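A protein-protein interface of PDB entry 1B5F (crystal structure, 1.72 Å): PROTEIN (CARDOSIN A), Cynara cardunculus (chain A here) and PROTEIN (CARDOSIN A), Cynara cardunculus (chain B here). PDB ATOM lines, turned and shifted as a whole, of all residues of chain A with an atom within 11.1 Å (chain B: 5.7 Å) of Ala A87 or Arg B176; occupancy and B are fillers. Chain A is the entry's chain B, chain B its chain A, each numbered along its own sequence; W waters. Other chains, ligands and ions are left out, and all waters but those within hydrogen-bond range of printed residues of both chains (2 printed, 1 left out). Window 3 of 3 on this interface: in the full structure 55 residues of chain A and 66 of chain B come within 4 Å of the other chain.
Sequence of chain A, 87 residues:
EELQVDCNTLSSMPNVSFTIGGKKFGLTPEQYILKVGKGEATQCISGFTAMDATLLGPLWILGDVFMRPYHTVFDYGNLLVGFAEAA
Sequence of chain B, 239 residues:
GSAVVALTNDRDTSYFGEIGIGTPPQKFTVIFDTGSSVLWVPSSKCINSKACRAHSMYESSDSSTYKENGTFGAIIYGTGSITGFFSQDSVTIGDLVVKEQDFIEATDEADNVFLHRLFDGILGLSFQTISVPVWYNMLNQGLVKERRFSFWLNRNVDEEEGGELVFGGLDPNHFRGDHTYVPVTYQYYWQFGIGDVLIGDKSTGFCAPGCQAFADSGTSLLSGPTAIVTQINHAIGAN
His A71 touches His B174.
Phe B175 touches His A71.
Phe B175 touches Ala A84.
Ala A84 touches Arg B176 (CB to O, 3.6 Å).
Ala A84 touches Asp B178 (CB to O, 3.8 Å).
Phe B175 touches Glu A85.
Ala A86 touches His B174.
Ala A87 touches Asn B173 (OXT to O, 3.7 Å).
Ala A87 touches Phe B175.
CB of Ala A87 touches CG of Arg B176 (3.8 Å).
O of Pro A69 is in hydrogen-bond range of N of Ala A86 (2.9 Å).
The backbone NH of His A71 lies within hydrogen-bond range of the backbone carbonyl oxygen of Ala A84 (2.8 Å).
Water W1 lies within hydrogen-bond range of the chain-end carboxylate of Ala A87 (2.7 Å) and a ring nitrogen (ND1) of His B174 (3.4 Å).
Water W2 lies within hydrogen-bond range of NZ of Lys A23 (2.8 Å), O of Asp B178 (2.8 Å) and O of Phe A83 (3.0 Å).
NE1 of Trp B152 sits at hydrogen-bond distance from OXT of Ala A87, 3.2 Å away.
The chain-end carboxylate of Ala A87 sits at hydrogen-bond distance from a ring nitrogen (ND1) of His B174 (2.9 Å).
NE of Arg B176 is in salt-bridge range of OE2 of Glu A85, at 3.7 Å.
Gln A31 touches none of the printed residues of chain B.
Pro A69 touches none of the printed residues of chain B.
Of the printed residues of chain B, His A71 touches His B174 and Phe B175.
Printed residues of chain B within 4 Å of Glu A85: Phe B175 and Arg B176.
Of the printed residues of chain B, Ala A86 touches His B174 (3.5 Å).
Ala A87 touches just these residues of chain B: Trp B152, Asn B173, His B174, Phe B175 and Arg B176.
Arg B176 touches just these residues of chain A: Ala A84, Glu A85 and Ala A87.
No residue of chain A comes within 4 Å of Gly B177.
Of the 8 printed residues of chain B, 6 touch a printed residue of chain A.
Printed residues of chain B that touch a printed residue of chain A: Trp B152, Asn B173, His B174, Phe B175, Arg B176 and Asp B178.
Hydrophobic or aromatic side chains of chain B that line the printed part of chain A: Trp B152, His B174 and Phe B175.
Among the printed residues, Asp or Glu carboxylates within 4 Å of a Lys or Arg side-chain nitrogen of the other chain: Glu A85 with Arg B176 (3.7 Å).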
ATOM      1  N   LYS A  23     -29.798  16.542 -19.989  1.00  0.00           N
ATOM      2  CA  LYS A  23     -29.139  16.507 -18.699  1.00  0.00           C
ATOM      3  C   LYS A  23     -30.086  16.897 -17.584  1.00  0.00           C
ATOM      4  O   LYS A  23     -30.907  17.787 -17.806  1.00  0.00           O
ATOM      5  CB  LYS A  23     -27.954  17.467 -18.778  1.00  0.00           C
ATOM      6  CG  LYS A  23     -27.115  17.555 -17.529  1.00  0.00           C
ATOM      7  CD  LYS A  23     -26.227  18.785 -17.480  1.00  0.00           C
ATOM      8  CE  LYS A  23     -24.884  18.508 -16.821  1.00  0.00           C
ATOM      9  NZ  LYS A  23     -24.487  19.575 -15.860  1.00  0.00           N
ATOM     10  N   PHE A  25     -31.165  18.963 -14.478  1.00  0.00           N
ATOM     11  CA  PHE A  25     -30.812  20.126 -13.674  1.00  0.00           C
ATOM     12  C   PHE A  25     -31.698  20.140 -12.426  1.00  0.00           C
ATOM     13  O   PHE A  25     -32.867  20.515 -12.550  1.00  0.00           O
ATOM     14  CB  PHE A  25     -30.987  21.425 -14.457  1.00  0.00           C
ATOM     15  CG  PHE A  25     -29.894  21.599 -15.508  1.00  0.00           C
ATOM     16  CD1 PHE A  25     -29.966  20.920 -16.705  1.00  0.00           C
ATOM     17  CD2 PHE A  25     -28.828  22.440 -15.235  1.00  0.00           C
ATOM     18  CE1 PHE A  25     -28.970  21.071 -17.654  1.00  0.00           C
ATOM     19  CE2 PHE A  25     -27.822  22.594 -16.169  1.00  0.00           C
ATOM     20  CZ  PHE A  25     -27.907  21.891 -17.352  1.00  0.00           C
ATOM     21  N   GLN A  31     -33.129  25.824  -2.503  1.00  0.00           N
ATOM     22  CA  GLN A  31     -33.115  26.618  -3.727  1.00  0.00           C
ATOM     23  C   GLN A  31     -34.522  26.952  -4.211  1.00  0.00           C
ATOM     24  O   GLN A  31     -34.750  28.076  -4.664  1.00  0.00           O
ATOM     25  CB  GLN A  31     -32.350  25.890  -4.844  1.00  0.00           C
ATOM     26  CG  GLN A  31     -30.855  25.793  -4.518  1.00  0.00           C
ATOM     27  CD  GLN A  31     -30.122  24.720  -5.283  1.00  0.00           C
ATOM     28  OE1 GLN A  31     -30.721  23.920  -5.993  1.00  0.00           O
ATOM     29  NE2 GLN A  31     -28.791  24.700  -5.137  1.00  0.00           N
ATOM     30  N   PHE A  66     -34.385  29.545 -10.539  1.00  0.00           N
ATOM     31  CA  PHE A  66     -33.530  28.663 -11.321  1.00  0.00           C
ATOM     32  C   PHE A  66     -32.183  29.297 -11.644  1.00  0.00           C
ATOM     33  O   PHE A  66     -31.166  28.598 -11.644  1.00  0.00           O
ATOM     34  CB  PHE A  66     -34.208  28.314 -12.640  1.00  0.00           C
ATOM     35  CG  PHE A  66     -33.513  27.233 -13.427  1.00  0.00           C
ATOM     36  CD1 PHE A  66     -33.866  25.911 -13.199  1.00  0.00           C
ATOM     37  CD2 PHE A  66     -32.546  27.504 -14.375  1.00  0.00           C
ATOM     38  CE1 PHE A  66     -33.255  24.889 -13.902  1.00  0.00           C
ATOM     39  CE2 PHE A  66     -31.919  26.482 -15.058  1.00  0.00           C
ATOM     40  CZ  PHE A  66     -32.266  25.174 -14.825  1.00  0.00           C
ATOM     41  N   MET A  67     -32.197  30.588 -11.954  1.00  0.00           N
ATOM     42  CA  MET A  67     -31.000  31.311 -12.357  1.00  0.00           C
ATOM     43  C   MET A  67     -30.041  31.641 -11.224  1.00  0.00           C
ATOM     44  O   MET A  67     -28.915  32.106 -11.474  1.00  0.00           O
ATOM     45  CB  MET A  67     -31.415  32.607 -13.120  1.00  0.00           C
ATOM     46  CG  MET A  67     -32.071  32.207 -14.443  1.00  0.00           C
ATOM     47  SD  MET A  67     -32.449  33.653 -15.465  1.00  0.00           S
ATOM     48  CE  MET A  67     -30.811  34.276 -15.827  1.00  0.00           C
ATOM     49  N   ARG A  68     -30.465  31.392  -9.987  1.00  0.00           N
ATOM     50  CA  ARG A  68     -29.551  31.455  -8.856  1.00  0.00           C
ATOM     51  C   ARG A  68     -28.658  30.215  -8.823  1.00  0.00           C
ATOM     52  O   ARG A  68     -27.425  30.397  -8.838  1.00  0.00           O
ATOM     53  CB  ARG A  68     -30.277  31.626  -7.505  1.00  0.00           C
ATOM     54  CG  ARG A  68     -30.573  33.029  -7.037  1.00  0.00           C
ATOM     55  CD  ARG A  68     -31.105  33.013  -5.600  1.00  0.00           C
ATOM     56  NE  ARG A  68     -32.473  32.514  -5.494  1.00  0.00           N
ATOM     57  CZ  ARG A  68     -33.594  33.205  -5.688  1.00  0.00           C
ATOM     58  NH1 ARG A  68     -33.577  34.491  -6.012  1.00  0.00           N
ATOM     59  NH2 ARG A  68     -34.785  32.645  -5.555  1.00  0.00           N
ATOM     60  N   PRO A  69     -29.125  28.984  -8.700  1.00  0.00           N
ATOM     61  CA  PRO A  69     -28.198  27.845  -8.644  1.00  0.00           C
ATOM     62  C   PRO A  69     -27.555  27.500  -9.974  1.00  0.00           C
ATOM     63  O   PRO A  69     -26.569  26.770  -9.971  1.00  0.00           O
ATOM     64  CB  PRO A  69     -29.057  26.665  -8.205  1.00  0.00           C
ATOM     65  CG  PRO A  69     -30.418  27.031  -8.641  1.00  0.00           C
ATOM     66  CD  PRO A  69     -30.503  28.517  -8.503  1.00  0.00           C
ATOM     67  N   TYR A  70     -28.091  28.026 -11.062  1.00  0.00           N
ATOM     68  CA  TYR A  70     -27.470  27.827 -12.379  1.00  0.00           C
ATOM     69  C   TYR A  70     -27.038  29.136 -13.001  1.00  0.00           C
ATOM     70  O   TYR A  70     -27.829  30.017 -13.349  1.00  0.00           O
ATOM     71  CB  TYR A  70     -28.472  27.040 -13.268  1.00  0.00           C
ATOM     72  CG  TYR A  70     -28.623  25.655 -12.673  1.00  0.00           C
ATOM     73  CD1 TYR A  70     -27.526  24.797 -12.663  1.00  0.00           C
ATOM     74  CD2 TYR A  70     -29.809  25.198 -12.115  1.00  0.00           C
ATOM     75  CE1 TYR A  70     -27.606  23.517 -12.122  1.00  0.00           C
ATOM     76  CE2 TYR A  70     -29.889  23.933 -11.574  1.00  0.00           C
ATOM     77  CZ  TYR A  70     -28.796  23.086 -11.571  1.00  0.00           C
ATOM     78  OH  TYR A  70     -28.887  21.816 -11.032  1.00  0.00           O
ATOM     79  N   HIS A  71     -25.732  29.309 -13.170  1.00  0.00           N
ATOM     80  CA  HIS A  71     -25.176  30.409 -13.932  1.00  0.00           C
ATOM     81  C   HIS A  71     -25.613  30.295 -15.387  1.00  0.00           C
ATOM     82  O   HIS A  71     -25.528  29.200 -15.958  1.00  0.00           O
ATOM     83  CB  HIS A  71     -23.655  30.301 -13.785  1.00  0.00           C
ATOM     84  CG  HIS A  71     -22.906  31.337 -14.551  1.00  0.00           C
ATOM     85  ND1 HIS A  71     -22.647  31.174 -15.886  1.00  0.00           N
ATOM     86  CD2 HIS A  71     -22.356  32.507 -14.207  1.00  0.00           C
ATOM     87  CE1 HIS A  71     -21.979  32.211 -16.345  1.00  0.00           C
ATOM     88  NE2 HIS A  71     -21.784  33.043 -15.332  1.00  0.00           N
ATOM     89  N   THR A  72     -26.077  31.373 -15.990  1.00  0.00           N
ATOM     90  CA  THR A  72     -26.671  31.351 -17.309  1.00  0.00           C
ATOM     91  C   THR A  72     -25.934  32.215 -18.318  1.00  0.00           C
ATOM     92  O   THR A  72     -25.587  33.357 -18.043  1.00  0.00           O
ATOM     93  CB  THR A  72     -28.146  31.829 -17.235  1.00  0.00           C
ATOM     94  OG1 THR A  72     -28.819  31.027 -16.247  1.00  0.00           O
ATOM     95  CG2 THR A  72     -28.857  31.565 -18.551  1.00  0.00           C
ATOM     96  N   VAL A  73     -25.699  31.609 -19.482  1.00  0.00           N
ATOM     97  CA  VAL A  73     -25.084  32.272 -20.610  1.00  0.00           C
ATOM     98  C   VAL A  73     -26.102  32.461 -21.728  1.00  0.00           C
ATOM     99  O   VAL A  73     -26.747  31.496 -22.132  1.00  0.00           O
ATOM    100  CB  VAL A  73     -23.900  31.483 -21.154  1.00  0.00           C
ATOM    101  CG1 VAL A  73     -23.441  32.090 -22.470  1.00  0.00           C
ATOM    102  CG2 VAL A  73     -22.774  31.487 -20.132  1.00  0.00           C
ATOM    103  N   GLY A  82     -27.055  28.546 -22.202  1.00  0.00           N
ATOM    104  CA  GLY A  82     -26.224  27.618 -21.476  1.00  0.00           C
ATOM    105  C   GLY A  82     -26.397  27.742 -19.980  1.00  0.00           C
ATOM    106  O   GLY A  82     -26.537  28.855 -19.469  1.00  0.00           O
ATOM    107  N   PHE A  83     -26.373  26.601 -19.313  1.00  0.00           N
ATOM    108  CA  PHE A  83     -26.443  26.544 -17.858  1.00  0.00           C
ATOM    109  C   PHE A  83     -25.294  25.714 -17.279  1.00  0.00           C
ATOM    110  O   PHE A  83     -24.973  24.659 -17.826  1.00  0.00           O
ATOM    111  CB  PHE A  83     -27.755  25.915 -17.423  1.00  0.00           C
ATOM    112  CG  PHE A  83     -29.005  26.637 -17.872  1.00  0.00           C
ATOM    113  CD1 PHE A  83     -29.333  27.852 -17.305  1.00  0.00           C
ATOM    114  CD2 PHE A  83     -29.827  26.079 -18.834  1.00  0.00           C
ATOM    115  CE1 PHE A  83     -30.475  28.529 -17.685  1.00  0.00           C
ATOM    116  CE2 PHE A  83     -30.948  26.783 -19.252  1.00  0.00           C
ATOM    117  CZ  PHE A  83     -31.256  28.001 -18.683  1.00  0.00           C
ATOM    118  N   ALA A  84     -24.720  26.222 -16.199  1.00  0.00           N
ATOM    119  CA  ALA A  84     -23.758  25.520 -15.368  1.00  0.00           C
ATOM    120  C   ALA A  84     -24.023  25.785 -13.890  1.00  0.00           C
ATOM    121  O   ALA A  84     -24.538  26.842 -13.525  1.00  0.00           O
ATOM    122  CB  ALA A  84     -22.323  25.952 -15.631  1.00  0.00           C
ATOM    123  N   GLU A  85     -23.615  24.852 -13.041  1.00  0.00           N
ATOM    124  CA  GLU A  85     -23.689  25.072 -11.602  1.00  0.00           C
ATOM    125  C   GLU A  85     -23.043  26.390 -11.210  1.00  0.00           C
ATOM    126  O   GLU A  85     -21.898  26.707 -11.515  1.00  0.00           O
ATOM    127  CB  GLU A  85     -23.004  23.891 -10.894  1.00  0.00           C
ATOM    128  CG  GLU A  85     -22.953  24.068  -9.381  1.00  0.00           C
ATOM    129  CD  GLU A  85     -21.989  23.065  -8.755  1.00  0.00           C
ATOM    130  OE1 GLU A  85     -21.591  22.105  -9.437  1.00  0.00           O
ATOM    131  OE2 GLU A  85     -21.616  23.246  -7.583  1.00  0.00           O
ATOM    132  N   ALA A  86     -23.796  27.233 -10.517  1.00  0.00           N
ATOM    133  CA  ALA A  86     -23.270  28.492 -10.050  1.00  0.00           C
ATOM    134  C   ALA A  86     -22.272  28.291  -8.895  1.00  0.00           C
ATOM    135  O   ALA A  86     -22.386  27.307  -8.172  1.00  0.00           O
ATOM    136  CB  ALA A  86     -24.386  29.412  -9.566  1.00  0.00           C
ATOM    137  N   ALA A  87     -21.340  29.231  -8.806  1.00  0.00           N
ATOM    138  CA  ALA A  87     -20.378  29.289  -7.711  1.00  0.00           C
ATOM    139  C   ALA A  87     -20.178  30.730  -7.275  1.00  0.00           C
ATOM    140  O   ALA A  87     -19.721  30.964  -6.143  1.00  0.00           O
ATOM    141  CB  ALA A  87     -19.055  28.666  -8.100  1.00  0.00           C
ATOM    142  OXT ALA A  87     -20.474  31.638  -8.074  1.00  0.00           O
ATOM    143  N   TRP B 152     -24.702  35.846 -13.160  1.00  0.00           N
ATOM    144  CA  TRP B 152     -24.567  35.215 -11.865  1.00  0.00           C
ATOM    145  C   TRP B 152     -25.560  35.895 -10.901  1.00  0.00           C
ATOM    146  O   TRP B 152     -25.462  37.112 -10.708  1.00  0.00           O
ATOM    147  CB  TRP B 152     -23.162  35.327 -11.282  1.00  0.00           C
ATOM    148  CG  TRP B 152     -23.071  34.798  -9.877  1.00  0.00           C
ATOM    149  CD1 TRP B 152     -23.339  33.531  -9.448  1.00  0.00           C
ATOM    150  CD2 TRP B 152     -22.682  35.548  -8.722  1.00  0.00           C
ATOM    151  NE1 TRP B 152     -23.141  33.445  -8.086  1.00  0.00           N
ATOM    152  CE2 TRP B 152     -22.737  34.668  -7.621  1.00  0.00           C
ATOM    153  CE3 TRP B 152     -22.292  36.872  -8.508  1.00  0.00           C
ATOM    154  CZ2 TRP B 152     -22.411  35.100  -6.336  1.00  0.00           C
ATOM    155  CZ3 TRP B 152     -21.968  37.300  -7.225  1.00  0.00           C
ATOM    156  CH2 TRP B 152     -22.031  36.404  -6.156  1.00  0.00           C
ATOM    157  N   PRO B 172     -15.550  33.064 -14.934  1.00  0.00           N
ATOM    158  CA  PRO B 172     -15.360  31.666 -14.525  1.00  0.00           C
ATOM    159  C   PRO B 172     -15.399  31.480 -13.023  1.00  0.00           C
ATOM    160  O   PRO B 172     -15.615  30.388 -12.506  1.00  0.00           O
ATOM    161  CB  PRO B 172     -13.961  31.317 -15.034  1.00  0.00           C
ATOM    162  CG  PRO B 172     -13.290  32.627 -15.257  1.00  0.00           C
ATOM    163  CD  PRO B 172     -14.363  33.622 -15.595  1.00  0.00           C
ATOM    164  N   ASN B 173     -15.215  32.585 -12.296  1.00  0.00           N
ATOM    165  CA  ASN B 173     -15.305  32.474 -10.849  1.00  0.00           C
ATOM    166  C   ASN B 173     -16.736  32.193 -10.402  1.00  0.00           C
ATOM    167  O   ASN B 173     -16.932  31.806  -9.253  1.00  0.00           O
ATOM    168  CB  ASN B 173     -14.825  33.746 -10.155  1.00  0.00           C
ATOM    169  CG  ASN B 173     -13.369  34.088 -10.360  1.00  0.00           C
ATOM    170  OD1 ASN B 173     -12.543  33.205 -10.569  1.00  0.00           O
ATOM    171  ND2 ASN B 173     -13.078  35.378 -10.288  1.00  0.00           N
ATOM    172  N   HIS B 174     -17.719  32.387 -11.278  1.00  0.00           N
ATOM    173  CA  HIS B 174     -19.088  32.152 -10.821  1.00  0.00           C
ATOM    174  C   HIS B 174     -19.790  30.935 -11.383  1.00  0.00           C
ATOM    175  O   HIS B 174     -21.025  30.848 -11.342  1.00  0.00           O
ATOM    176  CB  HIS B 174     -19.926  33.419 -11.135  1.00  0.00           C
ATOM    177  CG  HIS B 174     -19.540  34.503 -10.160  1.00  0.00           C
ATOM    178  ND1 HIS B 174     -19.523  34.275  -8.798  1.00  0.00           N
ATOM    179  CD2 HIS B 174     -19.165  35.789 -10.350  1.00  0.00           C
ATOM    180  CE1 HIS B 174     -19.147  35.393  -8.195  1.00  0.00           C
ATOM    181  NE2 HIS B 174     -18.922  36.320  -9.101  1.00  0.00           N
ATOM    182  N   PHE B 175     -19.035  29.974 -11.904  1.00  0.00           N
ATOM    183  CA  PHE B 175     -19.618  28.682 -12.244  1.00  0.00           C
ATOM    184  C   PHE B 175     -18.570  27.564 -12.113  1.00  0.00           C
ATOM    185  O   PHE B 175     -17.375  27.814 -12.042  1.00  0.00           O
ATOM    186  CB  PHE B 175     -20.259  28.629 -13.624  1.00  0.00           C
ATOM    187  CG  PHE B 175     -19.342  28.924 -14.788  1.00  0.00           C
ATOM    188  CD1 PHE B 175     -18.972  30.210 -15.125  1.00  0.00           C
ATOM    189  CD2 PHE B 175     -18.859  27.881 -15.558  1.00  0.00           C
ATOM    190  CE1 PHE B 175     -18.132  30.489 -16.193  1.00  0.00           C
ATOM    191  CE2 PHE B 175     -18.021  28.135 -16.620  1.00  0.00           C
ATOM    192  CZ  PHE B 175     -17.677  29.420 -16.962  1.00  0.00           C
ATOM    193  N   ARG B 176     -19.137  26.368 -12.055  1.00  0.00           N
ATOM    194  CA  ARG B 176     -18.317  25.167 -12.037  1.00  0.00           C
ATOM    195  C   ARG B 176     -18.753  24.273 -13.177  1.00  0.00           C
ATOM    196  O   ARG B 176     -19.945  24.257 -13.530  1.00  0.00           O
ATOM    197  CB  ARG B 176     -18.427  24.408 -10.712  1.00  0.00           C
ATOM    198  CG  ARG B 176     -18.189  25.299  -9.513  1.00  0.00           C
ATOM    199  CD  ARG B 176     -17.807  24.519  -8.270  1.00  0.00           C
ATOM    200  NE  ARG B 176     -18.040  23.085  -8.366  1.00  0.00           N
ATOM    201  CZ  ARG B 176     -17.172  22.083  -8.366  1.00  0.00           C
ATOM    202  NH1 ARG B 176     -15.856  22.267  -8.278  1.00  0.00           N
ATOM    203  NH2 ARG B 176     -17.648  20.840  -8.463  1.00  0.00           N
ATOM    204  N   GLY B 177     -17.779  23.539 -13.713  1.00  0.00           N
ATOM    205  CA  GLY B 177     -18.170  22.621 -14.795  1.00  0.00           C
ATOM    206  C   GLY B 177     -18.354  23.379 -16.096  1.00  0.00           C
ATOM    207  O   GLY B 177     -18.182  24.608 -16.122  1.00  0.00           O
ATOM    208  N   ASP B 178     -18.687  22.658 -17.170  1.00  0.00           N
ATOM    209  CA  ASP B 178     -19.015  23.275 -18.447  1.00  0.00           C
ATOM    210  C   ASP B 178     -20.501  23.663 -18.427  1.00  0.00           C
ATOM    211  O   ASP B 178     -21.259  22.961 -17.745  1.00  0.00           O
ATOM    212  CB  ASP B 178     -18.833  22.321 -19.610  1.00  0.00           C
ATOM    213  CG  ASP B 178     -17.473  22.122 -20.211  1.00  0.00           C
ATOM    214  OD1 ASP B 178     -16.492  22.773 -19.833  1.00  0.00           O
ATOM    215  OD2 ASP B 178     -17.381  21.258 -21.117  1.00  0.00           O
HETATM  216  O   HOH W   1     -19.132  33.527  -5.546  1.00  0.00           O
HETATM  217  O   HOH W   2     -23.851  21.865 -17.350  1.00  0.00           O
